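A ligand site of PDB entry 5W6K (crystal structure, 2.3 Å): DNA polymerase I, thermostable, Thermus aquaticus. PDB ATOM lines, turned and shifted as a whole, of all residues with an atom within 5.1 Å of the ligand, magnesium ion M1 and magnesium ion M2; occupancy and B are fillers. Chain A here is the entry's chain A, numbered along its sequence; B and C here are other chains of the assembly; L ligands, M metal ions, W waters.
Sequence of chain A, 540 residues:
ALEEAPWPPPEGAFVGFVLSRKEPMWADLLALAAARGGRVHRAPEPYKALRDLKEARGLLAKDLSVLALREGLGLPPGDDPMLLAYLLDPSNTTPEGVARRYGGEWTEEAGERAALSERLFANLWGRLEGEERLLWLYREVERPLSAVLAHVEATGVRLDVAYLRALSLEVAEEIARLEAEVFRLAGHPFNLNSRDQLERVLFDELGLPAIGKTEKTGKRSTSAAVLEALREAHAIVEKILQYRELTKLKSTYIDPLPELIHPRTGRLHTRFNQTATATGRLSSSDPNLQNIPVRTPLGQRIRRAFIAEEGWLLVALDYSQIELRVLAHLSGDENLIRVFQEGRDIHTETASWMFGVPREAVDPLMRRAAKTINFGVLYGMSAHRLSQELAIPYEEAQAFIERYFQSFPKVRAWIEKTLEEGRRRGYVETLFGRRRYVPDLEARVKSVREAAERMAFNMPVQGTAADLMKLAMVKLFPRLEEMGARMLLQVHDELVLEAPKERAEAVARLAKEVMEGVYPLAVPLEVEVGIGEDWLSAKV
The backbone carbonyl oxygen (O) of Tyr 319 binds magnesium ion M1.
O11 of the ligand is bound to magnesium ion M1, 2.0 Å away.
Magnesium ion M1 is bound by O12 of the ligand, 2.1 Å away.
An oxygen (O7) of the ligand is bound to magnesium ion M1, at 2.2 Å.
OD1 of Asp 318 binds magnesium ion M1, at 2.2 Å.
Magnesium ion M1 is bound by the side-chain carboxylate (OD2) of Asp 493, at 2.2 Å.
Magnesium ion M1 has six donor atoms within binding distance.
Ser 320 touches the ligand (CA to O9, 3.2 Å).
CZ of Phe 375 touches O2 of the ligand (3.0 Å).
Hydrophobic or aromatic side chains within 4 Å of the ligand: Ile 322, His 347 and Phe 375.
16 residues have an atom within 4 Å of the ligand: Arg 281, Asp 318, Tyr 319, Ser 320, Gln 321, Ile 322, Glu 323, His 347, Arg 367, Arg 368, Lys 371, Phe 375, Asp 493, 1WA 1 of chain B, DG 2 of chain B and DOC 12 of chain C.
The nearest printed residue that does not touch the ligand is Thr 372 (4.1 Å).
Water W1 bridges the side-chain carboxylate (OE1) of Glu 494 and the backbone carbonyl oxygen (O) of Val 491.
Water W5 lies within hydrogen-bond range of the backbone carbonyl oxygen of Asp 318 and an oxygen (O9) of the ligand.
Water W4 lies within hydrogen-bond range of an oxygen (O15) of the ligand (3.0 Å) and the side-chain amino group (NZ) of Lys 371 (3.1 Å).
Water W2 lies within hydrogen-bond range of NE2 of Gln 462 (2.8 Å), O1 of the ligand (2.9 Å) and OE1 of Glu 323 (3.0 Å).
The guanidinium group (NH2) of Arg 368 lies within salt-bridge range of OP2 of DOC 12 of chain C (2.8 Å).
The guanidinium group of Arg 281 sits at hydrogen-bond distance from O2 of DOC 12 of chain C (2.8 Å).
The side-chain carboxylate (OE1) of Glu 323 is in hydrogen-bond range of the side-chain hydroxyl (OH) of Tyr 379.
O2 of DOC 12 of chain C lies close to N2 of DG 2 of chain B, 2.7 Å away.
Residues that only touch magnesium ion M2: DOC 12 of chain C (3.8 Å).
Of the 22 residues printed, 3 come within 4 Å of magnesium ion M2.
The nearest printed residue that does not touch magnesium ion M2 is Glu 494 (4.3 Å).
Magnesium ion M2 is bound by OD1 of Asp 493 (2.0 Å), OD2 of Asp 318 (2.1 Å), O7 of the ligand (2.3 Å) and water W1 (2.3 Å).
Magnesium ion M2 has four donor atoms within binding distance.
Slightly farther from magnesium ion M2 lies water W3 (2.6 Å).
NH2 of Arg 281 is in hydrogen-bond range of O3 of the ligand (3.1 Å).
N2 of DG 2 of chain B sits close to O1 of the ligand, 3.4 Å away.
The backbone NH (N) of Gln 321 sits at hydrogen-bond distance from an oxygen (O9) of the ligand (3.0 Å).
O15 of the ligand is in salt-bridge range of NZ of Lys 371 (2.8 Å).
An oxygen (O8) of the ligand is in hydrogen-bond range of a ring nitrogen (NE2) of His 347, at 3.1 Å.
N4 of DOC 12 of chain C is in hydrogen-bond range of N3 of the ligand (3.4 Å).
An oxygen (O8) of the ligand sits at hydrogen-bond distance from the backbone NH (N) of Ile 322.
An oxygen (O2) of the ligand sits at hydrogen-bond distance from the backbone NH of Glu 323, 3.4 Å away.
An oxygen (O1) of the ligand sits at hydrogen-bond distance from N2 of 1WA 1 of chain B (2.7 Å).
NH1 of Arg 367 lies within salt-bridge range of O15 of the ligand, 2.9 Å away.
The guanidinium group (NH1) of Arg 368 sits at hydrogen-bond distance from an oxygen (O5) of the ligand, at 2.7 Å.
Three residues have an atom within 4 Å of magnesium ion M1: Asp 318, Tyr 319 and Asp 493.
Along chain A the residues within 4 Å of magnesium ion M1 span positions 318 to 493.
The nearest printed residue that does not touch magnesium ion M1 is Ser 320 (4.01 Å).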
ATOM      1  N   ARG A 281       2.552   6.881 -30.840  1.00  0.00           N
ATOM      2  CA  ARG A 281       3.958   6.834 -31.191  1.00  0.00           C
ATOM      3  C   ARG A 281       4.190   5.853 -32.335  1.00  0.00           C
ATOM      4  O   ARG A 281       3.389   4.955 -32.591  1.00  0.00           O
ATOM      5  CB  ARG A 281       4.805   6.416 -29.991  1.00  0.00           C
ATOM      6  CG  ARG A 281       5.282   7.535 -29.102  1.00  0.00           C
ATOM      7  CD  ARG A 281       6.331   7.025 -28.137  1.00  0.00           C
ATOM      8  NE  ARG A 281       6.889   8.064 -27.292  1.00  0.00           N
ATOM      9  CZ  ARG A 281       7.897   7.880 -26.451  1.00  0.00           C
ATOM     10  NH1 ARG A 281       8.457   6.672 -26.333  1.00  0.00           N
ATOM     11  NH2 ARG A 281       8.356   8.885 -25.716  1.00  0.00           N
ATOM     12  N   ASP A 318      16.356  17.163 -32.090  1.00  0.00           N
ATOM     13  CA  ASP A 318      15.656  16.597 -30.941  1.00  0.00           C
ATOM     14  C   ASP A 318      14.936  17.721 -30.197  1.00  0.00           C
ATOM     15  O   ASP A 318      15.562  18.698 -29.793  1.00  0.00           O
ATOM     16  CB  ASP A 318      16.656  15.897 -30.016  1.00  0.00           C
ATOM     17  CG  ASP A 318      15.974  15.113 -28.906  1.00  0.00           C
ATOM     18  OD1 ASP A 318      15.135  15.693 -28.183  1.00  0.00           O
ATOM     19  OD2 ASP A 318      16.290  13.910 -28.754  1.00  0.00           O
ATOM     20  N   TYR A 319      13.623  17.572 -30.041  1.00  0.00           N
ATOM     21  CA  TYR A 319      12.847  18.541 -29.266  1.00  0.00           C
ATOM     22  C   TYR A 319      13.320  18.544 -27.812  1.00  0.00           C
ATOM     23  O   TYR A 319      13.642  17.498 -27.245  1.00  0.00           O
ATOM     24  CB  TYR A 319      11.353  18.214 -29.318  1.00  0.00           C
ATOM     25  CG  TYR A 319      10.690  18.478 -30.650  1.00  0.00           C
ATOM     26  CD1 TYR A 319      10.271  19.751 -30.995  1.00  0.00           C
ATOM     27  CD2 TYR A 319      10.442  17.442 -31.540  1.00  0.00           C
ATOM     28  CE1 TYR A 319       9.648  19.999 -32.202  1.00  0.00           C
ATOM     29  CE2 TYR A 319       9.821  17.676 -32.745  1.00  0.00           C
ATOM     30  CZ  TYR A 319       9.430  18.955 -33.082  1.00  0.00           C
ATOM     31  OH  TYR A 319       8.807  19.183 -34.280  1.00  0.00           O
ATOM     32  N   SER A 320      13.342  19.730 -27.211  1.00  0.00           N
ATOM     33  CA  SER A 320      13.798  19.895 -25.832  1.00  0.00           C
ATOM     34  C   SER A 320      12.608  19.867 -24.888  1.00  0.00           C
ATOM     35  O   SER A 320      11.624  20.586 -25.104  1.00  0.00           O
ATOM     36  CB  SER A 320      14.575  21.204 -25.664  1.00  0.00           C
ATOM     37  OG  SER A 320      13.703  22.277 -25.372  1.00  0.00           O
ATOM     38  N   GLN A 321      12.696  19.042 -23.846  1.00  0.00           N
ATOM     39  CA  GLN A 321      11.667  18.969 -22.812  1.00  0.00           C
ATOM     40  C   GLN A 321      10.275  18.864 -23.440  1.00  0.00           C
ATOM     41  O   GLN A 321       9.326  19.535 -23.041  1.00  0.00           O
ATOM     42  CB  GLN A 321      11.746  20.172 -21.882  1.00  0.00           C
ATOM     43  CG  GLN A 321      13.164  20.558 -21.472  1.00  0.00           C
ATOM     44  CD  GLN A 321      13.203  21.818 -20.619  1.00  0.00           C
ATOM     45  OE1 GLN A 321      12.914  21.776 -19.422  1.00  0.00           O
ATOM     46  NE2 GLN A 321      13.552  22.933 -21.240  1.00  0.00           N
ATOM     47  N   ILE A 322      10.162  17.999 -24.456  1.00  0.00           N
ATOM     48  CA  ILE A 322       9.025  18.057 -25.358  1.00  0.00           C
ATOM     49  C   ILE A 322       7.719  17.856 -24.594  1.00  0.00           C
ATOM     50  O   ILE A 322       6.769  18.654 -24.724  1.00  0.00           O
ATOM     51  CB  ILE A 322       9.178  17.043 -26.502  1.00  0.00           C
ATOM     52  CG1 ILE A 322       7.971  17.093 -27.448  1.00  0.00           C
ATOM     53  CG2 ILE A 322       9.371  15.620 -25.987  1.00  0.00           C
ATOM     54  CD1 ILE A 322       7.734  18.462 -28.069  1.00  0.00           C
ATOM     55  N   GLU A 323       7.620  16.805 -23.788  1.00  0.00           N
ATOM     56  CA  GLU A 323       6.353  16.504 -23.132  1.00  0.00           C
ATOM     57  C   GLU A 323       6.052  17.481 -22.001  1.00  0.00           C
ATOM     58  O   GLU A 323       4.883  17.630 -21.620  1.00  0.00           O
ATOM     59  CB  GLU A 323       6.339  15.065 -22.621  1.00  0.00           C
ATOM     60  CG  GLU A 323       6.257  14.033 -23.749  1.00  0.00           C
ATOM     61  CD  GLU A 323       5.739  12.680 -23.306  1.00  0.00           C
ATOM     62  OE1 GLU A 323       5.276  12.558 -22.150  1.00  0.00           O
ATOM     63  OE2 GLU A 323       5.800  11.734 -24.113  1.00  0.00           O
ATOM     64  N   LEU A 324       7.070  18.156 -21.454  1.00  0.00           N
ATOM     65  CA  LEU A 324       6.806  19.219 -20.496  1.00  0.00           C
ATOM     66  C   LEU A 324       6.238  20.452 -21.204  1.00  0.00           C
ATOM     67  O   LEU A 324       5.312  21.090 -20.684  1.00  0.00           O
ATOM     68  CB  LEU A 324       8.078  19.582 -19.730  1.00  0.00           C
ATOM     69  CG  LEU A 324       8.663  18.504 -18.819  1.00  0.00           C
ATOM     70  CD1 LEU A 324       9.930  18.992 -18.144  1.00  0.00           C
ATOM     71  CD2 LEU A 324       7.645  18.046 -17.770  1.00  0.00           C
ATOM     72  N   HIS A 347      15.048  19.531 -16.565  1.00  0.00           N
ATOM     73  CA  HIS A 347      15.923  18.374 -16.397  1.00  0.00           C
ATOM     74  C   HIS A 347      17.255  18.772 -15.777  1.00  0.00           C
ATOM     75  O   HIS A 347      17.849  17.979 -15.032  1.00  0.00           O
ATOM     76  CB  HIS A 347      16.145  17.698 -17.758  1.00  0.00           C
ATOM     77  CG  HIS A 347      14.876  17.274 -18.431  1.00  0.00           C
ATOM     78  ND1 HIS A 347      13.716  17.008 -17.728  1.00  0.00           N
ATOM     79  CD2 HIS A 347      14.573  17.075 -19.737  1.00  0.00           C
ATOM     80  CE1 HIS A 347      12.761  16.667 -18.576  1.00  0.00           C
ATOM     81  NE2 HIS A 347      13.261  16.700 -19.803  1.00  0.00           N
ATOM     82  N   ARG A 367      21.667  14.453 -15.889  1.00  0.00           N
ATOM     83  CA  ARG A 367      20.433  15.045 -16.397  1.00  0.00           C
ATOM     84  C   ARG A 367      19.545  14.002 -17.056  1.00  0.00           C
ATOM     85  O   ARG A 367      18.318  14.101 -16.979  1.00  0.00           O
ATOM     86  CB  ARG A 367      20.762  16.174 -17.382  1.00  0.00           C
ATOM     87  CG  ARG A 367      19.550  16.866 -17.987  1.00  0.00           C
ATOM     88  CD  ARG A 367      19.984  18.037 -18.852  1.00  0.00           C
ATOM     89  NE  ARG A 367      18.847  18.674 -19.534  1.00  0.00           N
ATOM     90  CZ  ARG A 367      18.323  18.253 -20.679  1.00  0.00           C
ATOM     91  NH1 ARG A 367      18.815  17.189 -21.298  1.00  0.00           N
ATOM     92  NH2 ARG A 367      17.300  18.901 -21.215  1.00  0.00           N
ATOM     93  N   ARG A 368      20.141  13.014 -17.715  1.00  0.00           N
ATOM     94  CA  ARG A 368      19.367  11.884 -18.206  1.00  0.00           C
ATOM     95  C   ARG A 368      18.649  11.178 -17.061  1.00  0.00           C
ATOM     96  O   ARG A 368      17.516  10.718 -17.213  1.00  0.00           O
ATOM     97  CB  ARG A 368      20.283  10.909 -18.952  1.00  0.00           C
ATOM     98  CG  ARG A 368      19.631   9.605 -19.363  1.00  0.00           C
ATOM     99  CD  ARG A 368      19.618   9.432 -20.870  1.00  0.00           C
ATOM    100  NE  ARG A 368      18.911   8.216 -21.252  1.00  0.00           N
ATOM    101  CZ  ARG A 368      17.591   8.129 -21.429  1.00  0.00           C
ATOM    102  NH1 ARG A 368      16.822   9.195 -21.261  1.00  0.00           N
ATOM    103  NH2 ARG A 368      17.042   6.976 -21.774  1.00  0.00           N
ATOM    104  N   LYS A 371      15.427  12.998 -16.085  1.00  0.00           N
ATOM    105  CA  LYS A 371      14.265  12.716 -16.913  1.00  0.00           C
ATOM    106  C   LYS A 371      13.418  11.614 -16.300  1.00  0.00           C
ATOM    107  O   LYS A 371      12.188  11.745 -16.196  1.00  0.00           O
ATOM    108  CB  LYS A 371      14.693  12.343 -18.327  1.00  0.00           C
ATOM    109  CG  LYS A 371      15.450  13.439 -19.064  1.00  0.00           C
ATOM    110  CD  LYS A 371      15.702  13.051 -20.518  1.00  0.00           C
ATOM    111  CE  LYS A 371      16.697  13.996 -21.177  1.00  0.00           C
ATOM    112  NZ  LYS A 371      16.916  13.648 -22.614  1.00  0.00           N
ATOM    113  N   THR A 372      14.052  10.515 -15.892  1.00  0.00           N
ATOM    114  CA  THR A 372      13.332   9.456 -15.198  1.00  0.00           C
ATOM    115  C   THR A 372      12.596   9.998 -13.988  1.00  0.00           C
ATOM    116  O   THR A 372      11.449   9.634 -13.728  1.00  0.00           O
ATOM    117  CB  THR A 372      14.296   8.346 -14.790  1.00  0.00           C
ATOM    118  OG1 THR A 372      15.053   7.916 -15.927  1.00  0.00           O
ATOM    119  CG2 THR A 372      13.541   7.153 -14.217  1.00  0.00           C
ATOM    120  N   PHE A 375       9.787  12.846 -15.308  1.00  0.00           N
ATOM    121  CA  PHE A 375       8.692  12.160 -15.982  1.00  0.00           C
ATOM    122  C   PHE A 375       8.118  11.041 -15.105  1.00  0.00           C
ATOM    123  O   PHE A 375       6.916  10.768 -15.173  1.00  0.00           O
ATOM    124  CB  PHE A 375       9.173  11.602 -17.323  1.00  0.00           C
ATOM    125  CG  PHE A 375       9.481  12.666 -18.340  1.00  0.00           C
ATOM    126  CD1 PHE A 375       8.561  13.660 -18.614  1.00  0.00           C
ATOM    127  CD2 PHE A 375      10.701  12.694 -18.999  1.00  0.00           C
ATOM    128  CE1 PHE A 375       8.833  14.651 -19.540  1.00  0.00           C
ATOM    129  CE2 PHE A 375      10.977  13.677 -19.931  1.00  0.00           C
ATOM    130  CZ  PHE A 375      10.045  14.657 -20.193  1.00  0.00           C
ATOM    131  N   TYR A 379       3.987  11.151 -13.866  1.00  0.00           N
ATOM    132  CA  TYR A 379       2.973  10.171 -14.249  1.00  0.00           C
ATOM    133  C   TYR A 379       2.669   9.169 -13.140  1.00  0.00           C
ATOM    134  O   TYR A 379       2.486   7.976 -13.412  1.00  0.00           O
ATOM    135  CB  TYR A 379       3.411   9.449 -15.526  1.00  0.00           C
ATOM    136  CG  TYR A 379       3.563  10.371 -16.715  1.00  0.00           C
ATOM    137  CD1 TYR A 379       2.456  10.990 -17.274  1.00  0.00           C
ATOM    138  CD2 TYR A 379       4.805  10.606 -17.285  1.00  0.00           C
ATOM    139  CE1 TYR A 379       2.581  11.833 -18.363  1.00  0.00           C
ATOM    140  CE2 TYR A 379       4.933  11.442 -18.379  1.00  0.00           C
ATOM    141  CZ  TYR A 379       3.821  12.055 -18.918  1.00  0.00           C
ATOM    142  OH  TYR A 379       3.954  12.894 -19.996  1.00  0.00           O
ATOM    143  N   GLN A 462       1.931  12.241 -24.260  1.00  0.00           N
ATOM    144  CA  GLN A 462       2.834  11.529 -25.153  1.00  0.00           C
ATOM    145  C   GLN A 462       2.286  11.462 -26.567  1.00  0.00           C
ATOM    146  O   GLN A 462       3.065  11.457 -27.534  1.00  0.00           O
ATOM    147  CB  GLN A 462       3.080  10.116 -24.608  1.00  0.00           C
ATOM    148  CG  GLN A 462       3.966   9.238 -25.488  1.00  0.00           C
ATOM    149  CD  GLN A 462       4.183   7.862 -24.902  1.00  0.00           C
ATOM    150  OE1 GLN A 462       3.969   6.850 -25.567  1.00  0.00           O
ATOM    151  NE2 GLN A 462       4.595   7.820 -23.641  1.00  0.00           N
ATOM    152  N   VAL A 491      13.217   8.938 -33.776  1.00  0.00           N
ATOM    153  CA  VAL A 491      13.361   8.377 -32.445  1.00  0.00           C
ATOM    154  C   VAL A 491      12.409   9.116 -31.510  1.00  0.00           C
ATOM    155  O   VAL A 491      12.833   9.800 -30.577  1.00  0.00           O
ATOM    156  CB  VAL A 491      14.818   8.449 -31.942  1.00  0.00           C
ATOM    157  CG1 VAL A 491      14.974   7.685 -30.638  1.00  0.00           C
ATOM    158  CG2 VAL A 491      15.764   7.903 -33.005  1.00  0.00           C
ATOM    159  N   ASP A 493      10.958  11.725 -30.443  1.00  0.00           N
ATOM    160  CA  ASP A 493      11.003  13.180 -30.536  1.00  0.00           C
ATOM    161  C   ASP A 493      12.262  13.662 -31.237  1.00  0.00           C
ATOM    162  O   ASP A 493      12.647  14.826 -31.093  1.00  0.00           O
ATOM    163  CB  ASP A 493      10.895  13.812 -29.143  1.00  0.00           C
ATOM    164  CG  ASP A 493      12.228  13.888 -28.442  1.00  0.00           C
ATOM    165  OD1 ASP A 493      13.046  12.959 -28.605  1.00  0.00           O
ATOM    166  OD2 ASP A 493      12.461  14.880 -27.724  1.00  0.00           O
ATOM    167  N   GLU A 494      12.893  12.801 -32.020  1.00  0.00           N
ATOM    168  CA  GLU A 494      14.149  13.114 -32.681  1.00  0.00           C
ATOM    169  C   GLU A 494      14.104  12.649 -34.125  1.00  0.00           C
ATOM    170  O   GLU A 494      13.433  11.674 -34.454  1.00  0.00           O
ATOM    171  CB  GLU A 494      15.326  12.447 -31.940  1.00  0.00           C
ATOM    172  CG  GLU A 494      16.660  12.453 -32.681  1.00  0.00           C
ATOM    173  CD  GLU A 494      17.687  11.569 -32.016  1.00  0.00           C
ATOM    174  OE1 GLU A 494      17.435  11.116 -30.876  1.00  0.00           O
ATOM    175  OE2 GLU A 494      18.743  11.319 -32.634  1.00  0.00           O
ATOM    176  P   1WA B   1       4.960   3.291  -9.048  1.00  0.00           P
ATOM    177  N1  1WA B   1       9.052   7.630 -17.711  1.00  0.00           N
ATOM    178  C2  1WA B   1       7.761   7.870 -17.575  1.00  0.00           C
ATOM    179  N2  1WA B   1       7.143   8.502 -18.569  1.00  0.00           N
ATOM    180  N3  1WA B   1       6.966   7.537 -16.531  1.00  0.00           N
ATOM    181  C4  1WA B   1       7.609   6.923 -15.597  1.00  0.00           C
ATOM    182  N5  1WA B   1       8.919   6.626 -15.620  1.00  0.00           N
ATOM    183  C6  1WA B   1       9.732   6.989 -16.742  1.00  0.00           C
ATOM    184  O6  1WA B   1      10.886   6.712 -16.718  1.00  0.00           O
ATOM    185  C7  1WA B   1       9.274   5.963 -14.438  1.00  0.00           C
ATOM    186  C8  1WA B   1       8.164   5.865 -13.717  1.00  0.00           C
ATOM    187  N9  1WA B   1       7.129   6.462 -14.431  1.00  0.00           N
ATOM    188  C1' 1WA B   1       5.797   6.477 -13.817  1.00  0.00           C
ATOM    189  C2' 1WA B   1       4.667   5.878 -14.634  1.00  0.00           C
ATOM    190  C3' 1WA B   1       4.597   4.498 -13.975  1.00  0.00           C
ATOM    191  O3' 1WA B   1       3.315   3.950 -14.145  1.00  0.00           O
ATOM    192  C4' 1WA B   1       4.781   4.856 -12.509  1.00  0.00           C
ATOM    193  O4' 1WA B   1       5.841   5.846 -12.534  1.00  0.00           O
ATOM    194  C5' 1WA B   1       5.143   3.663 -11.637  1.00  0.00           C
ATOM    195  O5' 1WA B   1       5.444   4.120 -10.335  1.00  0.00           O
ATOM    196  OP1 1WA B   1       4.606   1.945  -9.504  1.00  0.00           O
ATOM    197  OP2 1WA B   1       6.004   3.557  -8.027  1.00  0.00           O
ATOM    198  P    DG B   2       3.101   2.761 -15.162  1.00  0.00           P
ATOM    199  OP1  DG B   2       1.770   2.187 -14.871  1.00  0.00           O
ATOM    200  OP2  DG B   2       4.314   1.917 -15.140  1.00  0.00           O
ATOM    201  O5'  DG B   2       3.041   3.489 -16.590  1.00  0.00           O
ATOM    202  C5'  DG B   2       1.965   4.355 -16.905  1.00  0.00           C
ATOM    203  C4'  DG B   2       2.224   5.124 -18.183  1.00  0.00           C
ATOM    204  O4'  DG B   2       3.401   5.966 -18.014  1.00  0.00           O
ATOM    205  C3'  DG B   2       2.529   4.268 -19.395  1.00  0.00           C
ATOM    206  O3'  DG B   2       1.322   3.837 -20.025  1.00  0.00           O
ATOM    207  C2'  DG B   2       3.343   5.213 -20.267  1.00  0.00           C
ATOM    208  C1'  DG B   2       4.120   6.023 -19.241  1.00  0.00           C
ATOM    209  N9   DG B   2       5.476   5.524 -19.020  1.00  0.00           N
ATOM    210  C8   DG B   2       5.928   4.822 -17.924  1.00  0.00           C
ATOM    211  N7   DG B   2       7.194   4.512 -18.004  1.00  0.00           N
ATOM    212  C5   DG B   2       7.597   5.028 -19.228  1.00  0.00           C
ATOM    213  C6   DG B   2       8.850   5.006 -19.859  1.00  0.00           C
ATOM    214  O6   DG B   2       9.906   4.493 -19.441  1.00  0.00           O
ATOM    215  N1   DG B   2       8.831   5.647 -21.089  1.00  0.00           N
ATOM    216  C2   DG B   2       7.725   6.246 -21.640  1.00  0.00           C
ATOM    217  N2   DG B   2       7.889   6.816 -22.838  1.00  0.00           N
ATOM    218  N3   DG B   2       6.538   6.278 -21.056  1.00  0.00           N
ATOM    219  C4   DG B   2       6.542   5.660 -19.861  1.00  0.00           C
ATOM    220  N1  DOC C  12      12.433   7.046 -24.454  1.00  0.00           N
ATOM    221  C2  DOC C  12      11.318   6.725 -23.726  1.00  0.00           C
ATOM    222  N3  DOC C  12      11.417   6.170 -22.529  1.00  0.00           N
ATOM    223  C4  DOC C  12      12.608   5.912 -22.005  1.00  0.00           C
ATOM    224  C5  DOC C  12      13.739   6.224 -22.711  1.00  0.00           C
ATOM    225  C6  DOC C  12      13.628   6.807 -23.952  1.00  0.00           C
ATOM    226  O2  DOC C  12      10.219   6.960 -24.191  1.00  0.00           O
ATOM    227  N4  DOC C  12      12.717   5.345 -20.803  1.00  0.00           N
ATOM    228  C1' DOC C  12      12.294   7.654 -25.757  1.00  0.00           C
ATOM    229  C2' DOC C  12      12.294   9.147 -25.652  1.00  0.00           C
ATOM    230  C3' DOC C  12      13.685   9.540 -26.038  1.00  0.00           C
ATOM    231  C4' DOC C  12      14.132   8.424 -26.935  1.00  0.00           C
ATOM    232  O4' DOC C  12      13.397   7.275 -26.559  1.00  0.00           O
ATOM    233  C5' DOC C  12      15.651   8.269 -26.858  1.00  0.00           C
ATOM    234  O5' DOC C  12      16.180   7.852 -25.624  1.00  0.00           O
ATOM    235  P   DOC C  12      17.748   7.769 -25.610  1.00  0.00           P
ATOM    236  OP1 DOC C  12      18.486   7.982 -26.886  1.00  0.00           O
ATOM    237  OP2 DOC C  12      18.231   7.492 -24.237  1.00  0.00           O
HETATM  238  N1  LIG L   1      13.774   9.297 -21.011  1.00  0.00           N
HETATM  239  C1  LIG L   1      10.311  10.110 -21.951  1.00  0.00           C
HETATM  240  C2  LIG L   1       9.549   9.490 -20.884  1.00  0.00           C
HETATM  241  O1  LIG L   1       8.367   9.486 -20.756  1.00  0.00           O
HETATM  242  N2  LIG L   1      10.330   8.827 -19.918  1.00  0.00           N
HETATM  243  C3  LIG L   1      11.676   8.728 -19.899  1.00  0.00           C
HETATM  244  N3  LIG L   1      12.198   8.042 -18.871  1.00  0.00           N
HETATM  245  C4  LIG L   1      12.367   9.334 -20.934  1.00  0.00           C
HETATM  246  C5  LIG L   1      11.650  10.022 -21.949  1.00  0.00           C
HETATM  247  C6  LIG L   1       9.412  10.798 -22.925  1.00  0.00           C
HETATM  248  C7  LIG L   1       9.086  12.203 -22.426  1.00  0.00           C
HETATM  249  C8  LIG L   1      10.140  13.003 -23.161  1.00  0.00           C
HETATM  250  O2  LIG L   1       9.911  14.401 -23.225  1.00  0.00           O
HETATM  251  C9  LIG L   1      10.164  12.310 -24.487  1.00  0.00           C
HETATM  252  O3  LIG L   1      10.019  10.967 -24.165  1.00  0.00           O
HETATM  253  C10 LIG L   1      11.442  12.580 -25.234  1.00  0.00           C
HETATM  254  O4  LIG L   1      12.543  12.185 -24.469  1.00  0.00           O
HETATM  255  O5  LIG L   1      14.409   8.786 -20.109  1.00  0.00           O
HETATM  256  O6  LIG L   1      14.281   9.769 -21.991  1.00  0.00           O
HETATM  257  O7  LIG L   1      14.112  13.725 -25.806  1.00  0.00           O
HETATM  258  O8  LIG L   1      12.004  15.862 -22.559  1.00  0.00           O
HETATM  259  O9  LIG L   1      15.661  18.328 -23.812  1.00  0.00           O
HETATM  260  O10 LIG L   1      15.094  12.245 -24.254  1.00  0.00           O
HETATM  261  O11 LIG L   1      12.575  15.847 -24.800  1.00  0.00           O
HETATM  262  O12 LIG L   1      15.653  16.364 -25.268  1.00  0.00           O
HETATM  263  O13 LIG L   1      13.649  14.085 -23.318  1.00  0.00           O
HETATM  264  O14 LIG L   1      14.373  16.426 -22.985  1.00  0.00           O
HETATM  265  O15 LIG L   1      16.966  16.353 -23.356  1.00  0.00           O
HETATM  266  P1  LIG L   1      13.855  13.061 -24.490  1.00  0.00           P
HETATM  267  P2  LIG L   1      13.169  15.552 -23.465  1.00  0.00           P
HETATM  268  P3  LIG L   1      15.628  16.846 -23.846  1.00  0.00           P
HETATM  269 MG    MG M   1      13.904  15.856 -26.337  1.00  0.00          MG
HETATM  270 MG    MG M   2      14.829  12.734 -27.712  1.00  0.00          MG
HETATM  271  O   HOH W   1      15.179  10.961 -29.203  1.00  0.00           O
HETATM  272  O   HOH W   2       5.648   9.602 -21.749  1.00  0.00           O
HETATM  273  O   HOH W   3      16.705  11.566 -26.250  1.00  0.00           O
HETATM  274  O   HOH W   4      17.606  14.424 -25.578  1.00  0.00           O
HETATM  275  O   HOH W   5      16.699  18.023 -27.045  1.00  0.00           O
